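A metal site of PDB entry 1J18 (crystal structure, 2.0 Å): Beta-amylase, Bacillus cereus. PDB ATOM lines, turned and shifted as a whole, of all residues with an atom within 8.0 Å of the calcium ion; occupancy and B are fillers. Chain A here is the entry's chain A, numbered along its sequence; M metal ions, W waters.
Merely in contact with the calcium ion: Lys 140.
Of the 17 residues printed, 6 come within 4 Å of the calcium ion.
Water W1 lies within hydrogen-bond range of the side-chain carboxylate (OE1) of Glu 56 (2.7 Å), the backbone carbonyl oxygen (O) of Glu 141 (2.8 Å) and the backbone NH (N) of Leu 145 (3.4 Å).
OD2 of Asp 60 lies within salt-bridge range of NZ of Lys 140, at 3.1 Å.
The side-chain amino group of Lys 140 is in salt-bridge range of the side-chain carboxylate of Glu 144.
The side-chain carboxylate (OE2) of Glu 141 is in salt-bridge range of the side-chain amino group (NZ) of Lys 140.
NE1 of Trp 106 sits at hydrogen-bond distance from O of Glu 56, at 2.8 Å.
NE1 of Trp 52 sits at hydrogen-bond distance from OE1 of Glu 56 (2.8 Å).
The calcium ion is bound by the side-chain carboxylate of Asp 60 (2.2 Å), the side-chain carboxylate of Glu 144 (2.4 Å), water W1 (2.5 Å), the side-chain carboxylate of Glu 141 (2.6 Å), the side-chain amide oxygen of Gln 61 (2.7 Å) and the side-chain carboxylate of Glu 56 (2.9 Å).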
ATOM      1  N   TRP A  52      28.906   4.885  -2.096  1.00  0.00           N
ATOM      2  CA  TRP A  52      28.409   4.509  -3.418  1.00  0.00           C
ATOM      3  C   TRP A  52      29.634   4.140  -4.243  1.00  0.00           C
ATOM      4  O   TRP A  52      29.606   3.193  -5.024  1.00  0.00           O
ATOM      5  CB  TRP A  52      27.683   5.713  -4.055  1.00  0.00           C
ATOM      6  CG  TRP A  52      26.968   5.404  -5.343  1.00  0.00           C
ATOM      7  CD1 TRP A  52      26.739   4.173  -5.886  1.00  0.00           C
ATOM      8  CD2 TRP A  52      26.349   6.354  -6.227  1.00  0.00           C
ATOM      9  NE1 TRP A  52      26.010   4.292  -7.055  1.00  0.00           N
ATOM     10  CE2 TRP A  52      25.756   5.623  -7.279  1.00  0.00           C
ATOM     11  CE3 TRP A  52      26.236   7.756  -6.219  1.00  0.00           C
ATOM     12  CZ2 TRP A  52      25.058   6.243  -8.328  1.00  0.00           C
ATOM     13  CZ3 TRP A  52      25.535   8.376  -7.253  1.00  0.00           C
ATOM     14  CH2 TRP A  52      24.955   7.618  -8.296  1.00  0.00           C
ATOM     15  N   GLU A  56      29.300   0.339  -6.083  1.00  0.00           N
ATOM     16  CA  GLU A  56      28.945   0.257  -7.495  1.00  0.00           C
ATOM     17  C   GLU A  56      30.022   0.947  -8.332  1.00  0.00           C
ATOM     18  O   GLU A  56      29.730   1.706  -9.245  1.00  0.00           O
ATOM     19  CB  GLU A  56      27.562   0.907  -7.709  1.00  0.00           C
ATOM     20  CG  GLU A  56      26.991   0.776  -9.123  1.00  0.00           C
ATOM     21  CD  GLU A  56      25.505   1.145  -9.190  1.00  0.00           C
ATOM     22  OE1 GLU A  56      25.085   2.111  -8.517  1.00  0.00           O
ATOM     23  OE2 GLU A  56      24.768   0.472  -9.937  1.00  0.00           O
ATOM     24  N   GLY A  59      30.662  -0.216 -12.657  1.00  0.00           N
ATOM     25  CA  GLY A  59      29.686   0.186 -13.639  1.00  0.00           C
ATOM     26  C   GLY A  59      28.252   0.035 -13.166  1.00  0.00           C
ATOM     27  O   GLY A  59      27.986  -0.548 -12.114  1.00  0.00           O
ATOM     28  N   ASP A  60      27.330   0.554 -13.967  1.00  0.00           N
ATOM     29  CA  ASP A  60      25.916   0.474 -13.634  1.00  0.00           C
ATOM     30  C   ASP A  60      25.492  -0.956 -13.335  1.00  0.00           C
ATOM     31  O   ASP A  60      25.744  -1.869 -14.116  1.00  0.00           O
ATOM     32  CB  ASP A  60      25.082   1.041 -14.799  1.00  0.00           C
ATOM     33  CG  ASP A  60      23.618   1.198 -14.439  1.00  0.00           C
ATOM     34  OD1 ASP A  60      23.326   1.751 -13.363  1.00  0.00           O
ATOM     35  OD2 ASP A  60      22.753   0.768 -15.230  1.00  0.00           O
ATOM     36  N   GLN A  61      24.847  -1.129 -12.184  1.00  0.00           N
ATOM     37  CA  GLN A  61      24.350  -2.426 -11.733  1.00  0.00           C
ATOM     38  C   GLN A  61      25.415  -3.467 -11.374  1.00  0.00           C
ATOM     39  O   GLN A  61      25.120  -4.653 -11.268  1.00  0.00           O
ATOM     40  CB  GLN A  61      23.400  -3.027 -12.783  1.00  0.00           C
ATOM     41  CG  GLN A  61      22.115  -2.226 -12.987  1.00  0.00           C
ATOM     42  CD  GLN A  61      21.454  -1.835 -11.675  1.00  0.00           C
ATOM     43  OE1 GLN A  61      21.895  -0.914 -10.994  1.00  0.00           O
ATOM     44  NE2 GLN A  61      20.390  -2.544 -11.309  1.00  0.00           N
ATOM     45  N   GLN A  62      26.655  -3.015 -11.185  1.00  0.00           N
ATOM     46  CA  GLN A  62      27.732  -3.906 -10.795  1.00  0.00           C
ATOM     47  C   GLN A  62      28.003  -3.647  -9.319  1.00  0.00           C
ATOM     48  O   GLN A  62      28.914  -2.903  -8.950  1.00  0.00           O
ATOM     49  CB  GLN A  62      28.976  -3.638 -11.646  1.00  0.00           C
ATOM     50  CG  GLN A  62      28.821  -4.083 -13.109  1.00  0.00           C
ATOM     51  CD  GLN A  62      30.028  -3.763 -13.960  1.00  0.00           C
ATOM     52  OE1 GLN A  62      31.151  -4.146 -13.633  1.00  0.00           O
ATOM     53  NE2 GLN A  62      29.810  -3.066 -15.068  1.00  0.00           N
ATOM     54  N   PHE A  63      27.174  -4.269  -8.481  1.00  0.00           N
ATOM     55  CA  PHE A  63      27.250  -4.086  -7.039  1.00  0.00           C
ATOM     56  C   PHE A  63      28.202  -4.971  -6.247  1.00  0.00           C
ATOM     57  O   PHE A  63      28.540  -6.091  -6.633  1.00  0.00           O
ATOM     58  CB  PHE A  63      25.842  -4.245  -6.446  1.00  0.00           C
ATOM     59  CG  PHE A  63      24.846  -3.278  -6.994  1.00  0.00           C
ATOM     60  CD1 PHE A  63      24.985  -1.910  -6.754  1.00  0.00           C
ATOM     61  CD2 PHE A  63      23.781  -3.720  -7.770  1.00  0.00           C
ATOM     62  CE1 PHE A  63      24.075  -1.001  -7.273  1.00  0.00           C
ATOM     63  CE2 PHE A  63      22.852  -2.816  -8.299  1.00  0.00           C
ATOM     64  CZ  PHE A  63      23.006  -1.455  -8.056  1.00  0.00           C
ATOM     65  N   TRP A 106      31.752   6.340 -13.513  1.00  0.00           N
ATOM     66  CA  TRP A 106      30.901   6.124 -14.682  1.00  0.00           C
ATOM     67  C   TRP A 106      29.614   6.944 -14.693  1.00  0.00           C
ATOM     68  O   TRP A 106      29.103   7.282 -15.766  1.00  0.00           O
ATOM     69  CB  TRP A 106      30.562   4.644 -14.835  1.00  0.00           C
ATOM     70  CG  TRP A 106      29.865   4.032 -13.658  1.00  0.00           C
ATOM     71  CD1 TRP A 106      30.437   3.366 -12.624  1.00  0.00           C
ATOM     72  CD2 TRP A 106      28.450   4.052 -13.397  1.00  0.00           C
ATOM     73  NE1 TRP A 106      29.471   2.958 -11.731  1.00  0.00           N
ATOM     74  CE2 TRP A 106      28.250   3.371 -12.183  1.00  0.00           C
ATOM     75  CE3 TRP A 106      27.340   4.578 -14.073  1.00  0.00           C
ATOM     76  CZ2 TRP A 106      26.972   3.194 -11.624  1.00  0.00           C
ATOM     77  CZ3 TRP A 106      26.071   4.403 -13.520  1.00  0.00           C
ATOM     78  CH2 TRP A 106      25.900   3.719 -12.301  1.00  0.00           C
ATOM     79  N   VAL A 107      29.081   7.259 -13.523  1.00  0.00           N
ATOM     80  CA  VAL A 107      27.835   8.012 -13.447  1.00  0.00           C
ATOM     81  C   VAL A 107      27.892   9.317 -14.256  1.00  0.00           C
ATOM     82  O   VAL A 107      26.888   9.731 -14.841  1.00  0.00           O
ATOM     83  CB  VAL A 107      27.454   8.342 -11.978  1.00  0.00           C
ATOM     84  CG1 VAL A 107      28.380   9.411 -11.413  1.00  0.00           C
ATOM     85  CG2 VAL A 107      26.011   8.791 -11.908  1.00  0.00           C
ATOM     86  N   GLN A 110      26.518   9.360 -17.871  1.00  0.00           N
ATOM     87  CA  GLN A 110      25.120   9.050 -18.109  1.00  0.00           C
ATOM     88  C   GLN A 110      24.429  10.183 -18.877  1.00  0.00           C
ATOM     89  O   GLN A 110      23.311  10.031 -19.353  1.00  0.00           O
ATOM     90  CB  GLN A 110      24.408   8.794 -16.784  1.00  0.00           C
ATOM     91  CG  GLN A 110      24.938   7.573 -16.059  1.00  0.00           C
ATOM     92  CD  GLN A 110      24.673   6.291 -16.824  1.00  0.00           C
ATOM     93  OE1 GLN A 110      23.536   5.831 -16.909  1.00  0.00           O
ATOM     94  NE2 GLN A 110      25.728   5.701 -17.385  1.00  0.00           N
ATOM     95  N   VAL A 137      17.973  10.801 -13.355  1.00  0.00           N
ATOM     96  CA  VAL A 137      19.134   9.981 -13.051  1.00  0.00           C
ATOM     97  C   VAL A 137      19.094   9.531 -11.593  1.00  0.00           C
ATOM     98  O   VAL A 137      19.401   8.375 -11.274  1.00  0.00           O
ATOM     99  CB  VAL A 137      20.444  10.762 -13.316  1.00  0.00           C
ATOM    100  CG1 VAL A 137      21.647   9.928 -12.890  1.00  0.00           C
ATOM    101  CG2 VAL A 137      20.541  11.101 -14.800  1.00  0.00           C
ATOM    102  N   LYS A 140      16.527   6.680 -10.982  1.00  0.00           N
ATOM    103  CA  LYS A 140      17.040   5.396 -11.459  1.00  0.00           C
ATOM    104  C   LYS A 140      18.155   4.851 -10.574  1.00  0.00           C
ATOM    105  O   LYS A 140      18.016   3.783  -9.974  1.00  0.00           O
ATOM    106  CB  LYS A 140      17.568   5.523 -12.888  1.00  0.00           C
ATOM    107  CG  LYS A 140      18.200   4.239 -13.409  1.00  0.00           C
ATOM    108  CD  LYS A 140      18.882   4.454 -14.754  1.00  0.00           C
ATOM    109  CE  LYS A 140      19.593   3.185 -15.196  1.00  0.00           C
ATOM    110  NZ  LYS A 140      20.668   2.798 -14.246  1.00  0.00           N
ATOM    111  N   GLU A 141      19.267   5.573 -10.508  1.00  0.00           N
ATOM    112  CA  GLU A 141      20.429   5.160  -9.722  1.00  0.00           C
ATOM    113  C   GLU A 141      20.140   4.924  -8.244  1.00  0.00           C
ATOM    114  O   GLU A 141      20.453   3.852  -7.715  1.00  0.00           O
ATOM    115  CB  GLU A 141      21.555   6.177  -9.869  1.00  0.00           C
ATOM    116  CG  GLU A 141      21.993   6.467 -11.300  1.00  0.00           C
ATOM    117  CD  GLU A 141      22.246   5.200 -12.110  1.00  0.00           C
ATOM    118  OE1 GLU A 141      22.838   4.257 -11.553  1.00  0.00           O
ATOM    119  OE2 GLU A 141      21.857   5.172 -13.291  1.00  0.00           O
ATOM    120  N   TYR A 142      19.557   5.907  -7.564  1.00  0.00           N
ATOM    121  CA  TYR A 142      19.264   5.719  -6.143  1.00  0.00           C
ATOM    122  C   TYR A 142      18.270   4.584  -5.959  1.00  0.00           C
ATOM    123  O   TYR A 142      18.398   3.771  -5.046  1.00  0.00           O
ATOM    124  CB  TYR A 142      18.730   7.014  -5.519  1.00  0.00           C
ATOM    125  CG  TYR A 142      19.773   8.089  -5.293  1.00  0.00           C
ATOM    126  CD1 TYR A 142      20.866   8.232  -6.149  1.00  0.00           C
ATOM    127  CD2 TYR A 142      19.634   9.024  -4.262  1.00  0.00           C
ATOM    128  CE1 TYR A 142      21.785   9.269  -6.002  1.00  0.00           C
ATOM    129  CE2 TYR A 142      20.540  10.078  -4.110  1.00  0.00           C
ATOM    130  CZ  TYR A 142      21.606  10.193  -4.978  1.00  0.00           C
ATOM    131  OH  TYR A 142      22.484  11.237  -4.867  1.00  0.00           O
ATOM    132  N   GLY A 143      17.269   4.529  -6.831  1.00  0.00           N
ATOM    133  CA  GLY A 143      16.284   3.465  -6.731  1.00  0.00           C
ATOM    134  C   GLY A 143      16.939   2.105  -6.796  1.00  0.00           C
ATOM    135  O   GLY A 143      16.654   1.226  -5.970  1.00  0.00           O
ATOM    136  N   GLU A 144      17.821   1.915  -7.775  1.00  0.00           N
ATOM    137  CA  GLU A 144      18.509   0.651  -7.970  1.00  0.00           C
ATOM    138  C   GLU A 144      19.462   0.334  -6.819  1.00  0.00           C
ATOM    139  O   GLU A 144      19.520  -0.800  -6.350  1.00  0.00           O
ATOM    140  CB  GLU A 144      19.292   0.677  -9.290  1.00  0.00           C
ATOM    141  CG  GLU A 144      18.410   0.918 -10.507  1.00  0.00           C
ATOM    142  CD  GLU A 144      19.207   1.032 -11.796  1.00  0.00           C
ATOM    143  OE1 GLU A 144      20.251   1.712 -11.785  1.00  0.00           O
ATOM    144  OE2 GLU A 144      18.774   0.460 -12.820  1.00  0.00           O
ATOM    145  N   LEU A 145      20.191   1.344  -6.354  1.00  0.00           N
ATOM    146  CA  LEU A 145      21.132   1.146  -5.248  1.00  0.00           C
ATOM    147  C   LEU A 145      20.381   0.752  -3.987  1.00  0.00           C
ATOM    148  O   LEU A 145      20.718  -0.257  -3.354  1.00  0.00           O
ATOM    149  CB  LEU A 145      21.942   2.427  -4.998  1.00  0.00           C
ATOM    150  CG  LEU A 145      23.042   2.354  -3.929  1.00  0.00           C
ATOM    151  CD1 LEU A 145      24.083   1.312  -4.328  1.00  0.00           C
ATOM    152  CD2 LEU A 145      23.695   3.723  -3.779  1.00  0.00           C
HETATM  153 CA    CA M   1      22.566   1.727 -11.249  1.00  0.00          CA
HETATM  154  O   HOH W   1      22.427   2.242  -8.819  1.00  0.00           O
